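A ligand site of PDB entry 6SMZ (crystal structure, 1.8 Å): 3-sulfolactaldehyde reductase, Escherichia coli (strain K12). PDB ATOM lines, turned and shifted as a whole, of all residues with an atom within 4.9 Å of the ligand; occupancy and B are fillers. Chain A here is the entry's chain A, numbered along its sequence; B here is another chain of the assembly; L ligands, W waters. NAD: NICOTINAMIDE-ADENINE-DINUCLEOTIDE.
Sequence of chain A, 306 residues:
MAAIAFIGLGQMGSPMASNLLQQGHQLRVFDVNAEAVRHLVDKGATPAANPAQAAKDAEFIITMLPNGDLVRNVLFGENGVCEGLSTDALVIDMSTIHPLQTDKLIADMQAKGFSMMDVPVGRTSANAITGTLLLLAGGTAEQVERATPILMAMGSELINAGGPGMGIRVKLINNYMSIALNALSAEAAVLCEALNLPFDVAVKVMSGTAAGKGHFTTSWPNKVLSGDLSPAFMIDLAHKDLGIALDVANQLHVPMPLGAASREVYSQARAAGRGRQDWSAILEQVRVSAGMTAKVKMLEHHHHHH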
ATOM      1  N   ILE A   7      26.541  12.150 -10.369  1.00  0.00           N
ATOM      2  CA  ILE A   7      25.735  11.116 -11.055  1.00  0.00           C
ATOM      3  C   ILE A   7      25.662   9.901 -10.143  1.00  0.00           C
ATOM      4  O   ILE A   7      26.716   9.309  -9.837  1.00  0.00           O
ATOM      5  CB  ILE A   7      26.318  10.784 -12.438  1.00  0.00           C
ATOM      6  CG1 ILE A   7      26.398  12.063 -13.302  1.00  0.00           C
ATOM      7  CG2 ILE A   7      25.495   9.665 -13.084  1.00  0.00           C
ATOM      8  CD1 ILE A   7      27.495  12.059 -14.251  1.00  0.00           C
ATOM      9  N   GLY A   8      24.460   9.533  -9.720  1.00  0.00           N
ATOM     10  CA  GLY A   8      24.231   8.501  -8.708  1.00  0.00           C
ATOM     11  C   GLY A   8      23.870   9.127  -7.373  1.00  0.00           C
ATOM     12  O   GLY A   8      24.803   9.540  -6.621  1.00  0.00           O
ATOM     13  N   LEU A   9      22.576   9.254  -7.092  1.00  0.00           N
ATOM     14  CA  LEU A   9      22.054   9.977  -5.895  1.00  0.00           C
ATOM     15  C   LEU A   9      21.345   9.002  -4.954  1.00  0.00           C
ATOM     16  O   LEU A   9      20.244   9.299  -4.449  1.00  0.00           O
ATOM     17  CB  LEU A   9      21.116  11.101  -6.351  1.00  0.00           C
ATOM     18  CG  LEU A   9      21.706  12.009  -7.415  1.00  0.00           C
ATOM     19  CD1 LEU A   9      20.661  12.980  -7.937  1.00  0.00           C
ATOM     20  CD2 LEU A   9      22.900  12.782  -6.875  1.00  0.00           C
ATOM     21  N   GLY A  10      22.020   7.887  -4.637  1.00  0.00           N
ATOM     22  CA  GLY A  10      21.435   6.835  -3.776  1.00  0.00           C
ATOM     23  C   GLY A  10      21.720   7.048  -2.300  1.00  0.00           C
ATOM     24  O   GLY A  10      21.870   8.211  -1.829  1.00  0.00           O
ATOM     25  N   GLN A  11      21.749   5.946  -1.542  1.00  0.00           N
ATOM     26  CA  GLN A  11      21.969   5.947  -0.072  1.00  0.00           C
ATOM     27  C   GLN A  11      23.247   6.737   0.256  1.00  0.00           C
ATOM     28  O   GLN A  11      23.263   7.433   1.278  1.00  0.00           O
ATOM     29  CB  GLN A  11      21.982   4.496   0.429  1.00  0.00           C
ATOM     30  CG  GLN A  11      21.918   4.416   1.939  1.00  0.00           C
ATOM     31  CD  GLN A  11      22.100   3.058   2.591  1.00  0.00           C
ATOM     32  OE1 GLN A  11      22.774   2.152   2.097  1.00  0.00           O
ATOM     33  NE2 GLN A  11      21.517   2.950   3.769  1.00  0.00           N
ATOM     34  N   MET A  12      24.303   6.601  -0.541  1.00  0.00           N
ATOM     35  CA  MET A  12      25.582   7.334  -0.330  1.00  0.00           C
ATOM     36  C   MET A  12      25.571   8.620  -1.144  1.00  0.00           C
ATOM     37  O   MET A  12      25.927   9.670  -0.608  1.00  0.00           O
ATOM     38  CB  MET A  12      26.816   6.494  -0.723  1.00  0.00           C
ATOM     39  CG  MET A  12      26.917   5.180   0.048  1.00  0.00           C
ATOM     40  SD  MET A  12      27.307   5.387   1.769  1.00  0.00           S
ATOM     41  CE  MET A  12      29.019   5.852   1.654  1.00  0.00           C
ATOM     42  N   GLY A  13      25.216   8.533  -2.432  1.00  0.00           N
ATOM     43  CA  GLY A  13      25.332   9.682  -3.342  1.00  0.00           C
ATOM     44  C   GLY A  13      24.513  10.884  -2.909  1.00  0.00           C
ATOM     45  O   GLY A  13      25.024  12.027  -3.021  1.00  0.00           O
ATOM     46  N   PHE A  30      22.304  14.077 -11.763  1.00  0.00           N
ATOM     47  CA  PHE A  30      21.530  13.117 -12.592  1.00  0.00           C
ATOM     48  C   PHE A  30      21.432  11.802 -11.833  1.00  0.00           C
ATOM     49  O   PHE A  30      22.411  11.332 -11.244  1.00  0.00           O
ATOM     50  CB  PHE A  30      22.130  12.932 -13.974  1.00  0.00           C
ATOM     51  CG  PHE A  30      21.380  11.894 -14.764  1.00  0.00           C
ATOM     52  CD1 PHE A  30      20.076  12.138 -15.140  1.00  0.00           C
ATOM     53  CD2 PHE A  30      21.922  10.610 -14.985  1.00  0.00           C
ATOM     54  CE1 PHE A  30      19.330  11.148 -15.769  1.00  0.00           C
ATOM     55  CE2 PHE A  30      21.171   9.664 -15.665  1.00  0.00           C
ATOM     56  CZ  PHE A  30      19.879   9.926 -16.029  1.00  0.00           C
ATOM     57  N   ASP A  31      20.241  11.228 -11.899  1.00  0.00           N
ATOM     58  CA  ASP A  31      19.946   9.856 -11.434  1.00  0.00           C
ATOM     59  C   ASP A  31      18.781   9.380 -12.308  1.00  0.00           C
ATOM     60  O   ASP A  31      17.958  10.212 -12.703  1.00  0.00           O
ATOM     61  CB  ASP A  31      19.605   9.817  -9.969  1.00  0.00           C
ATOM     62  CG  ASP A  31      19.655   8.425  -9.374  1.00  0.00           C
ATOM     63  OD1 ASP A  31      18.863   7.552  -9.809  1.00  0.00           O
ATOM     64  OD2 ASP A  31      20.496   8.228  -8.433  1.00  0.00           O
ATOM     65  N   VAL A  32      18.758   8.093 -12.643  1.00  0.00           N
ATOM     66  CA  VAL A  32      17.610   7.508 -13.417  1.00  0.00           C
ATOM     67  C   VAL A  32      16.340   7.589 -12.571  1.00  0.00           C
ATOM     68  O   VAL A  32      15.263   7.540 -13.167  1.00  0.00           O
ATOM     69  CB  VAL A  32      17.913   6.068 -13.876  1.00  0.00           C
ATOM     70  CG1 VAL A  32      18.992   6.040 -14.949  1.00  0.00           C
ATOM     71  CG2 VAL A  32      18.237   5.119 -12.730  1.00  0.00           C
ATOM     72  N   ASN A  33      16.455   7.710 -11.246  1.00  0.00           N
ATOM     73  CA  ASN A  33      15.333   7.891 -10.287  1.00  0.00           C
ATOM     74  C   ASN A  33      15.059   9.378 -10.139  1.00  0.00           C
ATOM     75  O   ASN A  33      15.829  10.099  -9.446  1.00  0.00           O
ATOM     76  CB  ASN A  33      15.621   7.172  -8.975  1.00  0.00           C
ATOM     77  CG  ASN A  33      14.621   7.482  -7.870  1.00  0.00           C
ATOM     78  OD1 ASN A  33      13.629   8.135  -8.097  1.00  0.00           O
ATOM     79  ND2 ASN A  33      14.873   7.019  -6.663  1.00  0.00           N
ATOM     80  N   ALA A  36      15.045  11.020  -6.636  1.00  0.00           N
ATOM     81  CA  ALA A  36      16.360  11.267  -6.005  1.00  0.00           C
ATOM     82  C   ALA A  36      16.908  12.604  -6.535  1.00  0.00           C
ATOM     83  O   ALA A  36      17.515  13.359  -5.770  1.00  0.00           O
ATOM     84  CB  ALA A  36      17.300  10.116  -6.285  1.00  0.00           C
ATOM     85  N   MET A  64      28.772   7.827  -8.318  1.00  0.00           N
ATOM     86  CA  MET A  64      28.577   6.995  -7.114  1.00  0.00           C
ATOM     87  C   MET A  64      27.518   5.948  -7.456  1.00  0.00           C
ATOM     88  O   MET A  64      26.331   6.195  -7.217  1.00  0.00           O
ATOM     89  CB  MET A  64      28.196   7.856  -5.897  1.00  0.00           C
ATOM     90  CG  MET A  64      28.234   7.143  -4.588  1.00  0.00           C
ATOM     91  SD  MET A  64      29.887   6.359  -4.344  1.00  0.00           S
ATOM     92  CE  MET A  64      29.867   5.991  -2.594  1.00  0.00           C
ATOM     93  N   LEU A  65      27.968   4.832  -8.041  1.00  0.00           N
ATOM     94  CA  LEU A  65      27.069   3.890  -8.744  1.00  0.00           C
ATOM     95  C   LEU A  65      27.306   2.470  -8.265  1.00  0.00           C
ATOM     96  O   LEU A  65      28.344   2.196  -7.673  1.00  0.00           O
ATOM     97  CB  LEU A  65      27.353   4.012 -10.231  1.00  0.00           C
ATOM     98  CG  LEU A  65      26.948   5.339 -10.861  1.00  0.00           C
ATOM     99  CD1 LEU A  65      27.566   5.499 -12.208  1.00  0.00           C
ATOM    100  CD2 LEU A  65      25.433   5.466 -10.924  1.00  0.00           C
ATOM    101  N   PRO A  66      26.323   1.561  -8.444  1.00  0.00           N
ATOM    102  CA  PRO A  66      26.428   0.226  -7.864  1.00  0.00           C
ATOM    103  C   PRO A  66      27.561  -0.667  -8.402  1.00  0.00           C
ATOM    104  O   PRO A  66      27.969  -1.558  -7.672  1.00  0.00           O
ATOM    105  CB  PRO A  66      25.061  -0.386  -8.222  1.00  0.00           C
ATOM    106  CG  PRO A  66      24.131   0.810  -8.321  1.00  0.00           C
ATOM    107  CD  PRO A  66      24.999   1.827  -9.042  1.00  0.00           C
ATOM    108  N   LEU A  70      27.855  -0.035 -14.819  1.00  0.00           N
ATOM    109  CA  LEU A  70      27.055   1.211 -14.774  1.00  0.00           C
ATOM    110  C   LEU A  70      27.997   2.416 -14.840  1.00  0.00           C
ATOM    111  O   LEU A  70      27.689   3.364 -15.573  1.00  0.00           O
ATOM    112  CB  LEU A  70      26.171   1.209 -13.529  1.00  0.00           C
ATOM    113  CG  LEU A  70      25.035   0.181 -13.544  1.00  0.00           C
ATOM    114  CD1 LEU A  70      24.275   0.168 -12.249  1.00  0.00           C
ATOM    115  CD2 LEU A  70      24.095   0.507 -14.682  1.00  0.00           C
ATOM    116  N   VAL A  74      27.658   5.119 -17.840  1.00  0.00           N
ATOM    117  CA  VAL A  74      27.481   6.562 -17.515  1.00  0.00           C
ATOM    118  C   VAL A  74      28.589   7.370 -18.181  1.00  0.00           C
ATOM    119  O   VAL A  74      28.301   8.502 -18.599  1.00  0.00           O
ATOM    120  CB  VAL A  74      27.389   6.740 -15.986  1.00  0.00           C
ATOM    121  CG1 VAL A  74      27.775   8.144 -15.549  1.00  0.00           C
ATOM    122  CG2 VAL A  74      26.015   6.372 -15.471  1.00  0.00           C
ATOM    123  N   SER A  95      32.706   5.084  -6.558  1.00  0.00           N
ATOM    124  CA  SER A  95      32.056   3.748  -6.513  1.00  0.00           C
ATOM    125  C   SER A  95      33.046   2.701  -6.015  1.00  0.00           C
ATOM    126  O   SER A  95      34.264   2.864  -6.235  1.00  0.00           O
ATOM    127  CB  SER A  95      31.493   3.371  -7.857  1.00  0.00           C
ATOM    128  OG  SER A  95      30.746   4.408  -8.447  1.00  0.00           O
ATOM    129  N   THR A  96      32.541   1.608  -5.419  1.00  0.00           N
ATOM    130  CA  THR A  96      33.384   0.405  -5.151  1.00  0.00           C
ATOM    131  C   THR A  96      33.140  -0.558  -6.317  1.00  0.00           C
ATOM    132  O   THR A  96      32.118  -1.209  -6.333  1.00  0.00           O
ATOM    133  CB  THR A  96      33.109  -0.265  -3.805  1.00  0.00           C
ATOM    134  OG1 THR A  96      33.302   0.721  -2.813  1.00  0.00           O
ATOM    135  CG2 THR A  96      34.018  -1.456  -3.581  1.00  0.00           C
ATOM    136  N   VAL A 121      35.082   5.189  -0.883  1.00  0.00           N
ATOM    137  CA  VAL A 121      34.913   5.676   0.494  1.00  0.00           C
ATOM    138  C   VAL A 121      34.712   4.503   1.441  1.00  0.00           C
ATOM    139  O   VAL A 121      34.111   3.492   1.065  1.00  0.00           O
ATOM    140  CB  VAL A 121      33.799   6.718   0.617  1.00  0.00           C
ATOM    141  CG1 VAL A 121      34.135   7.930  -0.232  1.00  0.00           C
ATOM    142  CG2 VAL A 121      32.457   6.122   0.243  1.00  0.00           C
ATOM    143  N   ARG A 123      33.361   3.656   5.616  1.00  0.00           N
ATOM    144  CA  ARG A 123      32.274   4.041   6.554  1.00  0.00           C
ATOM    145  C   ARG A 123      30.935   4.083   5.782  1.00  0.00           C
ATOM    146  O   ARG A 123      30.903   3.737   4.578  1.00  0.00           O
ATOM    147  CB  ARG A 123      32.615   5.337   7.305  1.00  0.00           C
ATOM    148  CG  ARG A 123      33.796   5.227   8.248  1.00  0.00           C
ATOM    149  CD  ARG A 123      34.257   6.597   8.793  1.00  0.00           C
ATOM    150  NE  ARG A 123      35.654   6.509   9.163  1.00  0.00           N
ATOM    151  CZ  ARG A 123      36.508   7.514   9.156  1.00  0.00           C
ATOM    152  NH1 ARG A 123      36.135   8.732   8.787  1.00  0.00           N
ATOM    153  NH2 ARG A 123      37.762   7.288   9.505  1.00  0.00           N
ATOM    154  N   THR A 124      29.845   4.395   6.463  1.00  0.00           N
ATOM    155  CA  THR A 124      28.519   3.981   5.963  1.00  0.00           C
ATOM    156  C   THR A 124      27.677   5.232   5.667  1.00  0.00           C
ATOM    157  O   THR A 124      28.229   6.378   5.719  1.00  0.00           O
ATOM    158  CB  THR A 124      27.916   2.975   6.934  1.00  0.00           C
ATOM    159  OG1 THR A 124      27.732   3.720   8.139  1.00  0.00           O
ATOM    160  CG2 THR A 124      28.810   1.771   7.134  1.00  0.00           C
ATOM    161  N   SER A 125      26.407   5.017   5.322  1.00  0.00           N
ATOM    162  CA  SER A 125      25.476   6.096   4.900  1.00  0.00           C
ATOM    163  C   SER A 125      25.300   7.129   6.031  1.00  0.00           C
ATOM    164  O   SER A 125      25.176   8.296   5.710  1.00  0.00           O
ATOM    165  CB  SER A 125      24.192   5.517   4.416  1.00  0.00           C
ATOM    166  OG  SER A 125      23.439   4.913   5.450  1.00  0.00           O
ATOM    167  N   LYS A 171      40.579   0.008  -0.936  1.00  0.00           N
ATOM    168  CA  LYS A 171      39.176  -0.224  -0.515  1.00  0.00           C
ATOM    169  C   LYS A 171      38.879  -1.734  -0.618  1.00  0.00           C
ATOM    170  O   LYS A 171      38.276  -2.300   0.307  1.00  0.00           O
ATOM    171  CB  LYS A 171      38.223   0.543  -1.421  1.00  0.00           C
ATOM    172  CG  LYS A 171      36.754   0.245  -1.238  1.00  0.00           C
ATOM    173  CD  LYS A 171      36.230   0.657   0.076  1.00  0.00           C
ATOM    174  CE  LYS A 171      34.751   0.405   0.241  1.00  0.00           C
ATOM    175  NZ  LYS A 171      34.348   0.764   1.619  1.00  0.00           N
ATOM    176  N   ALA B 232      23.816  -1.100   9.211  1.00  0.00           N
ATOM    177  CA  ALA B 232      24.884  -0.120   8.910  1.00  0.00           C
ATOM    178  C   ALA B 232      25.538  -0.500   7.583  1.00  0.00           C
ATOM    179  O   ALA B 232      25.759   0.349   6.734  1.00  0.00           O
ATOM    180  CB  ALA B 232      25.909  -0.088  10.039  1.00  0.00           C
ATOM    181  N   PHE B 233      25.885  -1.775   7.432  1.00  0.00           N
ATOM    182  CA  PHE B 233      26.491  -2.304   6.183  1.00  0.00           C
ATOM    183  C   PHE B 233      25.702  -3.558   5.819  1.00  0.00           C
ATOM    184  O   PHE B 233      25.798  -4.528   6.574  1.00  0.00           O
ATOM    185  CB  PHE B 233      27.986  -2.577   6.379  1.00  0.00           C
ATOM    186  CG  PHE B 233      28.723  -2.917   5.102  1.00  0.00           C
ATOM    187  CD1 PHE B 233      28.494  -2.194   3.934  1.00  0.00           C
ATOM    188  CD2 PHE B 233      29.686  -3.893   5.062  1.00  0.00           C
ATOM    189  CE1 PHE B 233      29.200  -2.475   2.776  1.00  0.00           C
ATOM    190  CE2 PHE B 233      30.393  -4.174   3.905  1.00  0.00           C
ATOM    191  CZ  PHE B 233      30.130  -3.490   2.752  1.00  0.00           C
ATOM    192  N   LEU B 237      25.407  -5.948   0.288  1.00  0.00           N
ATOM    193  CA  LEU B 237      26.566  -5.194  -0.225  1.00  0.00           C
ATOM    194  C   LEU B 237      27.856  -5.936   0.155  1.00  0.00           C
ATOM    195  O   LEU B 237      28.778  -5.970  -0.707  1.00  0.00           O
ATOM    196  CB  LEU B 237      26.590  -3.785   0.356  1.00  0.00           C
ATOM    197  CG  LEU B 237      27.718  -2.888  -0.192  1.00  0.00           C
ATOM    198  N   LYS B 240      28.255  -8.693  -2.295  1.00  0.00           N
ATOM    199  CA  LYS B 240      28.677  -8.173  -3.623  1.00  0.00           C
ATOM    200  C   LYS B 240      30.191  -7.867  -3.619  1.00  0.00           C
ATOM    201  O   LYS B 240      30.896  -8.276  -4.577  1.00  0.00           O
ATOM    202  CB  LYS B 240      27.869  -6.912  -4.003  1.00  0.00           C
ATOM    203  CG  LYS B 240      28.294  -6.261  -5.325  1.00  0.00           C
ATOM    204  CD  LYS B 240      27.424  -5.116  -5.814  1.00  0.00           C
ATOM    205  CE  LYS B 240      27.188  -4.045  -4.777  1.00  0.00           C
ATOM    206  NZ  LYS B 240      27.069  -2.679  -5.380  1.00  0.00           N
ATOM    207  N   ASP B 241      30.671  -7.181  -2.597  1.00  0.00           N
ATOM    208  CA  ASP B 241      32.091  -6.744  -2.513  1.00  0.00           C
ATOM    209  C   ASP B 241      32.990  -7.992  -2.397  1.00  0.00           C
ATOM    210  O   ASP B 241      34.047  -8.013  -3.005  1.00  0.00           O
ATOM    211  CB  ASP B 241      32.305  -5.765  -1.365  1.00  0.00           C
ATOM    212  CG  ASP B 241      31.865  -4.334  -1.676  1.00  0.00           C
ATOM    213  OD1 ASP B 241      31.308  -4.109  -2.806  1.00  0.00           O
ATOM    214  OD2 ASP B 241      32.035  -3.492  -0.768  1.00  0.00           O
HETATM  215  PA  NAD L   1      22.248   2.868  -4.157  1.00  0.00           P
HETATM  216  O1A NAD L   1      21.777   1.640  -4.893  1.00  0.00           O
HETATM  217  O2A NAD L   1      21.505   3.300  -2.943  1.00  0.00           O
HETATM  218  O5B NAD L   1      22.315   4.080  -5.210  1.00  0.00           O
HETATM  219  C5B NAD L   1      22.705   3.858  -6.568  1.00  0.00           C
HETATM  220  C4B NAD L   1      22.068   4.968  -7.353  1.00  0.00           C
HETATM  221  O4B NAD L   1      22.550   4.969  -8.706  1.00  0.00           O
HETATM  222  C3B NAD L   1      20.533   4.906  -7.401  1.00  0.00           C
HETATM  223  O3B NAD L   1      19.925   6.129  -6.991  1.00  0.00           O
HETATM  224  C2B NAD L   1      20.273   4.561  -8.868  1.00  0.00           C
HETATM  225  O2B NAD L   1      19.022   5.024  -9.286  1.00  0.00           O
HETATM  226  C1B NAD L   1      21.452   5.239  -9.558  1.00  0.00           C
HETATM  227  N9A NAD L   1      21.755   4.776 -10.906  1.00  0.00           N
HETATM  228  C8A NAD L   1      21.775   3.506 -11.394  1.00  0.00           C
HETATM  229  N7A NAD L   1      22.101   3.422 -12.662  1.00  0.00           N
HETATM  230  C5A NAD L   1      22.264   4.747 -13.049  1.00  0.00           C
HETATM  231  C6A NAD L   1      22.590   5.344 -14.281  1.00  0.00           C
HETATM  232  N6A NAD L   1      22.859   4.679 -15.404  1.00  0.00           N
HETATM  233  N1A NAD L   1      22.685   6.675 -14.286  1.00  0.00           N
HETATM  234  C2A NAD L   1      22.445   7.372 -13.173  1.00  0.00           C
HETATM  235  N3A NAD L   1      22.099   6.927 -11.975  1.00  0.00           N
HETATM  236  C4A NAD L   1      22.047   5.589 -11.970  1.00  0.00           C
HETATM  237  O3  NAD L   1      23.793   2.656  -3.807  1.00  0.00           O
HETATM  238  PN  NAD L   1      24.735   3.435  -2.766  1.00  0.00           P
HETATM  239  O1N NAD L   1      24.628   2.721  -1.466  1.00  0.00           O
HETATM  240  O2N NAD L   1      24.587   4.939  -2.887  1.00  0.00           O
HETATM  241  O5D NAD L   1      26.121   2.955  -3.358  1.00  0.00           O
HETATM  242  C5D NAD L   1      26.783   3.401  -4.520  1.00  0.00           C
HETATM  243  C4D NAD L   1      28.211   2.945  -4.334  1.00  0.00           C
HETATM  244  O4D NAD L   1      28.567   3.214  -2.963  1.00  0.00           O
HETATM  245  C3D NAD L   1      28.518   1.454  -4.547  1.00  0.00           C
HETATM  246  O3D NAD L   1      29.666   1.308  -5.364  1.00  0.00           O
HETATM  247  C2D NAD L   1      28.808   0.949  -3.132  1.00  0.00           C
HETATM  248  O2D NAD L   1      29.670  -0.185  -3.037  1.00  0.00           O
HETATM  249  C1D NAD L   1      29.447   2.195  -2.519  1.00  0.00           C
HETATM  250  N1N NAD L   1      29.437   2.207  -1.033  1.00  0.00           N
HETATM  251  C2N NAD L   1      28.262   1.952  -0.358  1.00  0.00           C
HETATM  252  C3N NAD L   1      28.220   1.900   1.048  1.00  0.00           C
HETATM  253  C7N NAD L   1      26.896   1.655   1.758  1.00  0.00           C
HETATM  254  O7N NAD L   1      26.916   1.299   2.943  1.00  0.00           O
HETATM  255  N7N NAD L   1      25.751   1.884   1.113  1.00  0.00           N
HETATM  256  C4N NAD L   1      29.456   2.101   1.759  1.00  0.00           C
HETATM  257  C5N NAD L   1      30.573   2.585   1.083  1.00  0.00           C
HETATM  258  C6N NAD L   1      30.595   2.528  -0.315  1.00  0.00           C
HETATM  259  O   HOH W   1      25.160   2.405   4.881  1.00  0.00           O
HETATM  260  O   HOH W   2      23.981  -1.053   0.707  1.00  0.00           O
HETATM  261  O   HOH W   3      20.783   0.871  -9.449  1.00  0.00           O
HETATM  262  O   HOH W   4      24.838  -0.904   3.313  1.00  0.00           O
HETATM  263  O   HOH W   5      31.529  -0.952  -0.929  1.00  0.00           O
HETATM  264  O   HOH W   6      19.903   1.398  -6.681  1.00  0.00           O
HETATM  265  O   HOH W   7      32.027  -0.471   1.774  1.00  0.00           O
HETATM  266  O   HOH W   8      23.064  -0.604  -5.106  1.00  0.00           O
HETATM  267  O   HOH W   9      24.669   6.706  -4.951  1.00  0.00           O
HETATM  268  O   HOH W  10      20.816   1.350 -13.862  1.00  0.00           O
HETATM  269  O   HOH W  11      23.581   5.749 -18.339  1.00  0.00           O
HETATM  270  O   HOH W  12      17.457   5.850  -5.980  1.00  0.00           O
HETATM  271  O   HOH W  13      17.035   3.277  -9.508  1.00  0.00           O
HETATM  272  O   HOH W  14      33.007   3.460  -2.451  1.00  0.00           O
HETATM  273  O   HOH W  15      30.312  -2.356  -4.468  1.00  0.00           O
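Water W15 lies within hydrogen-bond range of the side-chain carboxylate (OD1) of Asp 241 of chain B (2.6 Å), an oxygen (O2D) of the ligand (2.7 Å), the backbone carbonyl oxygen (O) of Thr 96 (2.8 Å) and the side-chain amino group (NZ) of Lys 240 of chain B (3.4 Å).
Water W12 lies within hydrogen-bond range of O3B of the ligand and ND2 of Asn 33.
Water W9 lies within hydrogen-bond range of an oxygen (O2N) of the ligand (2.7 Å), the backbone carbonyl oxygen of Met 64 (2.9 Å), the backbone NH of Gly 10 (2.9 Å), the backbone NH of Gly 13 (3.2 Å) and the backbone carbonyl oxygen of Gly 8 (3.3 Å).
Water W1 lies within hydrogen-bond range of the backbone carbonyl oxygen (O) of Ala 232 of chain B (2.8 Å), an oxygen (O7N) of the ligand (2.8 Å) and the backbone NH (N) of Ser 125 (2.9 Å).
Water W5 lies within hydrogen-bond range of the side-chain carboxylate of Asp 241 of chain B (2.6 Å), an oxygen (O2D) of the ligand (2.9 Å) and the side-chain hydroxyl of Thr 96 (3.1 Å).
Water W14 lies within hydrogen-bond range of OG1 of Thr 96 (2.8 Å) and N of Val 121 (3.1 Å).
The side-chain carboxylate (OD2) of Asp 31 lies within hydrogen-bond range of the backbone NH (N) of Leu 9, 2.7 Å away.
OD1 of Asp 31 lies within hydrogen-bond range of N of Asn 33 (2.8 Å).
The side-chain hydroxyl of Ser 95 sits at hydrogen-bond distance from the backbone NH of Leu 65, at 2.8 Å.
SD of Met 12 is in hydrogen-bond range of N of Ser 125 (3.7 Å).
The side-chain hydroxyl (OG) of Ser 125 sits at hydrogen-bond distance from the side-chain amide nitrogen (NE2) of Gln 11 (3.2 Å).
The backbone carbonyl oxygen (O) of Ile 7 sits at hydrogen-bond distance from the backbone NH (N) of Met 64 (3.0 Å).
N of Gly 8 sits at hydrogen-bond distance from O of Phe 30.
O of Pro 66 lies within hydrogen-bond range of NZ of Lys 240 of chain B.
OD1 of Asp 31 is in hydrogen-bond range of O2B of the ligand (2.6 Å).
An oxygen (O3D) of the ligand is in hydrogen-bond range of the backbone carbonyl oxygen (O) of Leu 65, at 2.8 Å.
N of Met 12 is in hydrogen-bond range of O2N of the ligand (2.9 Å).
O3D of the ligand is in hydrogen-bond range of N of Thr 96, at 2.9 Å.
The backbone NH (N) of Gln 11 sits at hydrogen-bond distance from an oxygen (O2A) of the ligand (3.0 Å).
N7N of the ligand is in hydrogen-bond range of OE1 of Gln 11, at 3.1 Å.
The side-chain sulfur of Met 64 lies close to an oxygen (O4D) of the ligand (3.7 Å).
Merely in contact with the ligand: Ile 7, Gly 8, Leu 9, Gly 10, Gly 13, Phe 30, Val 32, Pro 66, Leu 70, Val 74, Ser 95, Val 121, Arg 123 and Phe 233 of chain B.
Hydrophobic or aromatic side chains that line the ligand: Ile 7, Met 12, Phe 30, Val 32, Met 64, Leu 65, Pro 66, Leu 70, Val 74 and Phe 233 of chain B.
Of the 29 residues printed, 20 come within 4 Å of the ligand.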
